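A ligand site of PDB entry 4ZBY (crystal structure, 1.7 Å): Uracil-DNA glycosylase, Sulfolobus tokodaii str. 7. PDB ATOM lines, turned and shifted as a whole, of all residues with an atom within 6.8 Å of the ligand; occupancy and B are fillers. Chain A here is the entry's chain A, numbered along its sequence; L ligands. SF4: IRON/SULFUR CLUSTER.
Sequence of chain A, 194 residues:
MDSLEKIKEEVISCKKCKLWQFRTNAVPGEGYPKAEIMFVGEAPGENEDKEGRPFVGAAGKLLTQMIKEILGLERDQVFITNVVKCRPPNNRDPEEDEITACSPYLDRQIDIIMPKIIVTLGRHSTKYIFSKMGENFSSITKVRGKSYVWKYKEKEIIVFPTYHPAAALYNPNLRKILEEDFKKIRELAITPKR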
ATOM      1  N   GLU A  10       3.494   8.085   0.916  1.00  0.00           N
ATOM      2  CA  GLU A  10       4.084   7.225  -0.104  1.00  0.00           C
ATOM      3  C   GLU A  10       3.939   5.775   0.270  1.00  0.00           C
ATOM      4  O   GLU A  10       3.591   4.969  -0.584  1.00  0.00           O
ATOM      5  CB  GLU A  10       5.561   7.554  -0.313  1.00  0.00           C
ATOM      6  CG  GLU A  10       5.791   8.933  -0.927  1.00  0.00           C
ATOM      7  CD  GLU A  10       7.240   9.193  -1.204  1.00  0.00           C
ATOM      8  OE1 GLU A  10       7.997   8.205  -1.349  1.00  0.00           O
ATOM      9  OE2 GLU A  10       7.647  10.390  -1.283  1.00  0.00           O
ATOM     10  N   VAL A  11       4.229   5.447   1.527  1.00  0.00           N
ATOM     11  CA  VAL A  11       4.142   4.054   1.994  1.00  0.00           C
ATOM     12  C   VAL A  11       2.713   3.532   1.882  1.00  0.00           C
ATOM     13  O   VAL A  11       2.482   2.422   1.420  1.00  0.00           O
ATOM     14  CB  VAL A  11       4.641   3.912   3.421  1.00  0.00           C
ATOM     15  CG1 VAL A  11       4.195   2.564   4.050  1.00  0.00           C
ATOM     16  CG2 VAL A  11       6.170   4.034   3.463  1.00  0.00           C
ATOM     17  N   ILE A  12       1.752   4.354   2.285  1.00  0.00           N
ATOM     18  CA  ILE A  12       0.354   3.909   2.323  1.00  0.00           C
ATOM     19  C   ILE A  12      -0.158   3.520   0.932  1.00  0.00           C
ATOM     20  O   ILE A  12      -1.007   2.618   0.799  1.00  0.00           O
ATOM     21  CB  ILE A  12      -0.520   4.991   2.952  1.00  0.00           C
ATOM     22  CG1 ILE A  12      -0.349   4.928   4.486  1.00  0.00           C
ATOM     23  CG2 ILE A  12      -1.983   4.841   2.529  1.00  0.00           C
ATOM     24  CD1 ILE A  12      -1.001   6.101   5.196  1.00  0.00           C
ATOM     25  N   SER A  13       0.383   4.143  -0.110  1.00  0.00           N
ATOM     26  CA  SER A  13      -0.015   3.791  -1.469  1.00  0.00           C
ATOM     27  C   SER A  13       1.055   3.077  -2.278  1.00  0.00           C
ATOM     28  O   SER A  13       0.922   2.944  -3.493  1.00  0.00           O
ATOM     29  CB  SER A  13      -0.433   5.031  -2.245  1.00  0.00           C
ATOM     30  OG  SER A  13      -1.608   5.576  -1.685  1.00  0.00           O
ATOM     31  N   CYS A  14       2.110   2.639  -1.595  1.00  0.00           N
ATOM     32  CA  CYS A  14       3.296   2.100  -2.260  1.00  0.00           C
ATOM     33  C   CYS A  14       3.072   0.774  -2.962  1.00  0.00           C
ATOM     34  O   CYS A  14       2.449  -0.134  -2.410  1.00  0.00           O
ATOM     35  CB  CYS A  14       4.422   1.925  -1.243  1.00  0.00           C
ATOM     36  SG  CYS A  14       5.982   1.449  -2.000  1.00  0.00           S
ATOM     37  N   LYS A  15       3.608   0.645  -4.176  1.00  0.00           N
ATOM     38  CA  LYS A  15       3.601  -0.647  -4.843  1.00  0.00           C
ATOM     39  C   LYS A  15       4.976  -0.973  -5.408  1.00  0.00           C
ATOM     40  O   LYS A  15       5.110  -1.577  -6.460  1.00  0.00           O
ATOM     41  CB  LYS A  15       2.528  -0.666  -5.936  1.00  0.00           C
ATOM     42  CG  LYS A  15       1.155  -0.364  -5.370  1.00  0.00           C
ATOM     43  CD  LYS A  15       0.056  -0.365  -6.406  1.00  0.00           C
ATOM     44  CE  LYS A  15      -1.282  -0.044  -5.756  1.00  0.00           C
ATOM     45  NZ  LYS A  15      -2.384  -0.067  -6.759  1.00  0.00           N
ATOM     46  N   LYS A  16       5.998  -0.613  -4.655  1.00  0.00           N
ATOM     47  CA  LYS A  16       7.374  -0.749  -5.121  1.00  0.00           C
ATOM     48  C   LYS A  16       7.944  -2.157  -4.940  1.00  0.00           C
ATOM     49  O   LYS A  16       8.988  -2.447  -5.495  1.00  0.00           O
ATOM     50  CB  LYS A  16       8.263   0.280  -4.429  1.00  0.00           C
ATOM     51  CG  LYS A  16       8.024   1.692  -4.903  1.00  0.00           C
ATOM     52  CD  LYS A  16       8.906   2.648  -4.132  1.00  0.00           C
ATOM     53  CE  LYS A  16       9.007   3.972  -4.856  1.00  0.00           C
ATOM     54  NZ  LYS A  16       9.751   4.940  -4.025  1.00  0.00           N
ATOM     55  N   CYS A  17       7.292  -3.012  -4.163  1.00  0.00           N
ATOM     56  CA  CYS A  17       7.659  -4.428  -4.201  1.00  0.00           C
ATOM     57  C   CYS A  17       6.414  -5.297  -4.186  1.00  0.00           C
ATOM     58  O   CYS A  17       5.304  -4.792  -4.070  1.00  0.00           O
ATOM     59  CB  CYS A  17       8.591  -4.801  -3.036  1.00  0.00           C
ATOM     60  SG  CYS A  17       7.774  -5.066  -1.464  1.00  0.00           S
ATOM     61  N   LYS A  18       6.582  -6.604  -4.341  1.00  0.00           N
ATOM     62  CA  LYS A  18       5.412  -7.464  -4.514  1.00  0.00           C
ATOM     63  C   LYS A  18       4.554  -7.612  -3.259  1.00  0.00           C
ATOM     64  O   LYS A  18       3.448  -8.163  -3.325  1.00  0.00           O
ATOM     65  CB  LYS A  18       5.850  -8.849  -5.020  1.00  0.00           C
ATOM     66  CG  LYS A  18       6.753  -9.596  -4.058  1.00  0.00           C
ATOM     67  CD  LYS A  18       7.218 -10.928  -4.657  1.00  0.00           C
ATOM     68  CE  LYS A  18       8.159 -11.646  -3.706  1.00  0.00           C
ATOM     69  NZ  LYS A  18       9.391 -10.854  -3.368  1.00  0.00           N
ATOM     70  N   LEU A  19       5.010  -7.103  -2.133  1.00  0.00           N
ATOM     71  CA  LEU A  19       4.243  -7.255  -0.902  1.00  0.00           C
ATOM     72  C   LEU A  19       2.933  -6.466  -0.908  1.00  0.00           C
ATOM     73  O   LEU A  19       2.031  -6.788  -0.122  1.00  0.00           O
ATOM     74  CB  LEU A  19       5.063  -6.832   0.314  1.00  0.00           C
ATOM     75  CG  LEU A  19       6.301  -7.696   0.582  1.00  0.00           C
ATOM     76  CD1 LEU A  19       7.024  -7.346   1.877  1.00  0.00           C
ATOM     77  CD2 LEU A  19       5.875  -9.176   0.532  1.00  0.00           C
ATOM     78  N   TRP A  20       2.820  -5.452  -1.766  1.00  0.00           N
ATOM     79  CA  TRP A  20       1.634  -4.608  -1.730  1.00  0.00           C
ATOM     80  C   TRP A  20       0.373  -5.422  -2.007  1.00  0.00           C
ATOM     81  O   TRP A  20      -0.675  -5.130  -1.474  1.00  0.00           O
ATOM     82  CB  TRP A  20       1.741  -3.432  -2.722  1.00  0.00           C
ATOM     83  CG  TRP A  20       1.420  -3.813  -4.152  1.00  0.00           C
ATOM     84  CD1 TRP A  20       2.286  -4.240  -5.105  1.00  0.00           C
ATOM     85  CD2 TRP A  20       0.128  -3.798  -4.765  1.00  0.00           C
ATOM     86  NE1 TRP A  20       1.620  -4.488  -6.278  1.00  0.00           N
ATOM     87  CE2 TRP A  20       0.290  -4.217  -6.100  1.00  0.00           C
ATOM     88  CE3 TRP A  20      -1.157  -3.454  -4.325  1.00  0.00           C
ATOM     89  CZ2 TRP A  20      -0.773  -4.313  -6.990  1.00  0.00           C
ATOM     90  CZ3 TRP A  20      -2.201  -3.552  -5.200  1.00  0.00           C
ATOM     91  CH2 TRP A  20      -2.010  -3.965  -6.525  1.00  0.00           C
ATOM     92  N   GLN A  21       0.489  -6.460  -2.851  1.00  0.00           N
ATOM     93  CA  GLN A  21      -0.668  -7.189  -3.289  1.00  0.00           C
ATOM     94  C   GLN A  21      -1.405  -7.941  -2.182  1.00  0.00           C
ATOM     95  O   GLN A  21      -2.576  -8.268  -2.339  1.00  0.00           O
ATOM     96  CB  GLN A  21      -0.270  -8.175  -4.408  1.00  0.00           C
ATOM     97  CG  GLN A  21       0.588  -9.324  -3.917  1.00  0.00           C
ATOM     98  CD  GLN A  21       1.141 -10.169  -5.062  1.00  0.00           C
ATOM     99  OE1 GLN A  21       0.435 -11.005  -5.642  1.00  0.00           O
ATOM    100  NE2 GLN A  21       2.415  -9.961  -5.381  1.00  0.00           N
ATOM    101  N   ARG A  23      -1.589  -6.927   1.147  1.00  0.00           N
ATOM    102  CA  ARG A  23      -1.838  -6.153   2.351  1.00  0.00           C
ATOM    103  C   ARG A  23      -3.272  -5.644   2.477  1.00  0.00           C
ATOM    104  O   ARG A  23      -4.011  -5.496   1.479  1.00  0.00           O
ATOM    105  CB  ARG A  23      -0.852  -4.971   2.453  1.00  0.00           C
ATOM    106  CG  ARG A  23      -1.250  -3.779   1.618  1.00  0.00           C
ATOM    107  CD  ARG A  23      -0.182  -2.690   1.615  1.00  0.00           C
ATOM    108  NE  ARG A  23      -0.536  -1.711   0.595  1.00  0.00           N
ATOM    109  CZ  ARG A  23       0.344  -1.079  -0.193  1.00  0.00           C
ATOM    110  NH1 ARG A  23       1.648  -1.325  -0.068  1.00  0.00           N
ATOM    111  NH2 ARG A  23      -0.078  -0.224  -1.104  1.00  0.00           N
ATOM    112  N   ALA A  26      -0.541  -0.819   4.584  1.00  0.00           N
ATOM    113  CA  ALA A  26       0.906  -0.649   4.757  1.00  0.00           C
ATOM    114  C   ALA A  26       1.101  -0.032   6.129  1.00  0.00           C
ATOM    115  O   ALA A  26       0.172   0.598   6.651  1.00  0.00           O
ATOM    116  CB  ALA A  26       1.491   0.253   3.673  1.00  0.00           C
ATOM    117  N   VAL A  27       2.298  -0.166   6.693  1.00  0.00           N
ATOM    118  CA  VAL A  27       2.573   0.310   8.049  1.00  0.00           C
ATOM    119  C   VAL A  27       3.823   1.180   8.047  1.00  0.00           C
ATOM    120  O   VAL A  27       4.953   0.652   8.202  1.00  0.00           O
ATOM    121  CB  VAL A  27       2.777  -0.900   9.016  1.00  0.00           C
ATOM    122  CG1 VAL A  27       2.971  -0.436  10.447  1.00  0.00           C
ATOM    123  CG2 VAL A  27       1.556  -1.871   8.952  1.00  0.00           C
ATOM    124  N   VAL A  83      11.904  -2.267   9.092  1.00  0.00           N
ATOM    125  CA  VAL A  83      12.725  -2.146   7.895  1.00  0.00           C
ATOM    126  C   VAL A  83      11.869  -2.410   6.635  1.00  0.00           C
ATOM    127  O   VAL A  83      12.103  -1.792   5.581  1.00  0.00           O
ATOM    128  CB  VAL A  83      13.947  -3.085   7.952  1.00  0.00           C
ATOM    129  CG1 VAL A  83      13.512  -4.544   8.051  1.00  0.00           C
ATOM    130  CG2 VAL A  83      14.870  -2.868   6.763  1.00  0.00           C
ATOM    131  N   VAL A  84      10.873  -3.284   6.743  1.00  0.00           N
ATOM    132  CA  VAL A  84       9.922  -3.521   5.669  1.00  0.00           C
ATOM    133  C   VAL A  84       8.545  -3.136   6.191  1.00  0.00           C
ATOM    134  O   VAL A  84       8.214  -3.422   7.344  1.00  0.00           O
ATOM    135  CB  VAL A  84       9.959  -4.990   5.207  1.00  0.00           C
ATOM    136  CG1 VAL A  84       8.755  -5.345   4.355  1.00  0.00           C
ATOM    137  CG2 VAL A  84      11.256  -5.223   4.427  1.00  0.00           C
ATOM    138  N   LYS A  85       7.750  -2.477   5.352  1.00  0.00           N
ATOM    139  CA  LYS A  85       6.536  -1.875   5.870  1.00  0.00           C
ATOM    140  C   LYS A  85       5.207  -2.533   5.462  1.00  0.00           C
ATOM    141  O   LYS A  85       4.120  -2.072   5.844  1.00  0.00           O
ATOM    142  CB  LYS A  85       6.575  -0.383   5.531  1.00  0.00           C
ATOM    143  CG  LYS A  85       7.704   0.306   6.333  1.00  0.00           C
ATOM    144  CD  LYS A  85       8.120   1.611   5.691  1.00  0.00           C
ATOM    145  CE  LYS A  85       8.747   2.543   6.699  1.00  0.00           C
ATOM    146  NZ  LYS A  85      10.020   2.052   7.314  1.00  0.00           N
ATOM    147  N   CYS A  86       5.291  -3.659   4.741  1.00  0.00           N
ATOM    148  CA  CYS A  86       4.108  -4.472   4.484  1.00  0.00           C
ATOM    149  C   CYS A  86       4.321  -5.883   4.984  1.00  0.00           C
ATOM    150  O   CYS A  86       5.439  -6.360   5.047  1.00  0.00           O
ATOM    151  CB  CYS A  86       3.789  -4.513   2.994  1.00  0.00           C
ATOM    152  SG  CYS A  86       3.373  -2.839   2.404  1.00  0.00           S
ATOM    153  N   ARG A  87       3.235  -6.514   5.390  1.00  0.00           N
ATOM    154  CA  ARG A  87       3.261  -7.898   5.900  1.00  0.00           C
ATOM    155  C   ARG A  87       3.599  -8.926   4.826  1.00  0.00           C
ATOM    156  O   ARG A  87       2.871  -9.079   3.865  1.00  0.00           O
ATOM    157  CB  ARG A  87       1.891  -8.265   6.507  1.00  0.00           C
ATOM    158  CG  ARG A  87       1.833  -9.632   7.169  1.00  0.00           C
ATOM    159  CD  ARG A  87       0.393 -10.093   7.311  1.00  0.00           C
ATOM    160  NE  ARG A  87       0.301 -11.275   8.150  1.00  0.00           N
ATOM    161  CZ  ARG A  87      -0.822 -11.982   8.338  1.00  0.00           C
ATOM    162  NH1 ARG A  87      -0.805 -13.047   9.118  1.00  0.00           N
ATOM    163  NH2 ARG A  87      -1.944 -11.613   7.744  1.00  0.00           N
ATOM    164  N   GLU A  98      12.840  -7.317  -1.194  1.00  0.00           N
ATOM    165  CA  GLU A  98      11.820  -6.539  -0.513  1.00  0.00           C
ATOM    166  C   GLU A  98      12.484  -5.561   0.468  1.00  0.00           C
ATOM    167  O   GLU A  98      12.073  -4.405   0.578  1.00  0.00           O
ATOM    168  CB  GLU A  98      10.816  -7.466   0.191  1.00  0.00           C
ATOM    169  CG  GLU A  98       9.961  -8.238  -0.808  1.00  0.00           C
ATOM    170  CD  GLU A  98       9.352  -9.513  -0.247  1.00  0.00           C
ATOM    171  OE1 GLU A  98       9.569  -9.816   0.947  1.00  0.00           O
ATOM    172  OE2 GLU A  98       8.629 -10.169  -1.012  1.00  0.00           O
ATOM    173  N   ALA A 101      13.941  -2.854  -1.641  1.00  0.00           N
ATOM    174  CA  ALA A 101      12.907  -1.947  -2.173  1.00  0.00           C
ATOM    175  C   ALA A 101      12.362  -1.001  -1.118  1.00  0.00           C
ATOM    176  O   ALA A 101      12.082   0.166  -1.413  1.00  0.00           O
ATOM    177  CB  ALA A 101      11.765  -2.751  -2.781  1.00  0.00           C
ATOM    178  N   CYS A 102      12.185  -1.491   0.101  1.00  0.00           N
ATOM    179  CA  CYS A 102      11.491  -0.732   1.121  1.00  0.00           C
ATOM    180  C   CYS A 102      12.425   0.087   2.004  1.00  0.00           C
ATOM    181  O   CYS A 102      12.034   1.108   2.552  1.00  0.00           O
ATOM    182  CB  CYS A 102      10.683  -1.673   2.012  1.00  0.00           C
ATOM    183  SG  CYS A 102       9.399  -0.834   2.973  1.00  0.00           S
ATOM    184  N   SER A 103      13.644  -0.394   2.179  1.00  0.00           N
ATOM    185  CA  SER A 103      14.517   0.258   3.158  1.00  0.00           C
ATOM    186  C   SER A 103      14.810   1.753   2.893  1.00  0.00           C
ATOM    187  O   SER A 103      15.085   2.470   3.849  1.00  0.00           O
ATOM    188  CB  SER A 103      15.822  -0.527   3.297  1.00  0.00           C
ATOM    189  OG  SER A 103      16.540  -0.593   2.099  1.00  0.00           O
ATOM    190  N   TYR A 105      12.779   4.002   2.612  1.00  0.00           N
ATOM    191  CA  TYR A 105      11.832   4.715   3.484  1.00  0.00           C
ATOM    192  C   TYR A 105      12.401   4.845   4.873  1.00  0.00           C
ATOM    193  O   TYR A 105      12.335   5.911   5.475  1.00  0.00           O
ATOM    194  CB  TYR A 105      10.485   3.984   3.562  1.00  0.00           C
ATOM    195  CG  TYR A 105       9.651   4.015   2.283  1.00  0.00           C
ATOM    196  CD1 TYR A 105       9.442   5.207   1.606  1.00  0.00           C
ATOM    197  CD2 TYR A 105       9.058   2.842   1.784  1.00  0.00           C
ATOM    198  CE1 TYR A 105       8.651   5.270   0.483  1.00  0.00           C
ATOM    199  CE2 TYR A 105       8.265   2.883   0.641  1.00  0.00           C
ATOM    200  CZ  TYR A 105       8.063   4.123  -0.005  1.00  0.00           C
ATOM    201  OH  TYR A 105       7.300   4.208  -1.134  1.00  0.00           O
HETATM  202 FE1  SF4 L   1       7.098  -3.067  -0.559  1.00  0.00          FE
HETATM  203 FE2  SF4 L   1       6.312  -0.515  -0.675  1.00  0.00          FE
HETATM  204 FE3  SF4 L   1       5.192  -2.187   1.127  1.00  0.00          FE
HETATM  205 FE4  SF4 L   1       7.712  -1.378   1.427  1.00  0.00          FE
HETATM  206  S1  SF4 L   1       5.859  -0.077   1.537  1.00  0.00           S
HETATM  207  S2  SF4 L   1       6.947  -3.471   1.686  1.00  0.00           S
HETATM  208  S3  SF4 L   1       8.429  -1.262  -0.739  1.00  0.00           S
HETATM  209  S4  SF4 L   1       5.079  -2.345  -1.178  1.00  0.00           S
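Lys 16 touches the ligand (N to S4, 3.99 Å).
CD1 of Leu 19 touches S2 of the ligand (3.9 Å).
Trp 20 touches the ligand.
Val 84 touches the ligand.
Lys 85 touches the ligand.
Ala 101 touches the ligand (C to S3, 3.96 Å).
Tyr 105 touches the ligand (CE2 to S1, 3.9 Å).
SG of Cys 14 lies close to N of Lys 16.
The backbone carbonyl oxygen of Cys 14 is in hydrogen-bond range of the guanidinium group of Arg 23 (2.7 Å).
O of Lys 85 is in hydrogen-bond range of N of Val 27 (2.8 Å).
The guanidinium group (NH1) of Arg 23 lies close to the side-chain sulfur (SG) of Cys 86.
SG of Cys 17 sits close to N of Leu 19 (3.5 Å).
The side-chain hydroxyl (OH) of Tyr 105 sits close to the side-chain sulfur (SG) of Cys 14.
The backbone NH (N) of Lys 85 sits close to the side-chain sulfur (SG) of Cys 102 (3.3 Å).
The side-chain sulfur (SG) of Cys 86 is bound to an iron atom (FE3) of the ligand (2.3 Å).
SG of Cys 14 is bound to FE2 of the ligand (2.4 Å).
The side-chain sulfur (SG) of Cys 17 binds an iron atom (FE1) of the ligand.
N of Cys 86 lies close to S2 of the ligand (3.5 Å).
The guanidinium group of Arg 23 sits close to a sulfur (S4) of the ligand, 3.7 Å away.
SG of Cys 102 binds FE4 of the ligand (2.4 Å).
The backbone NH (N) of Cys 17 lies close to a sulfur (S4) of the ligand, 3.8 Å away.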
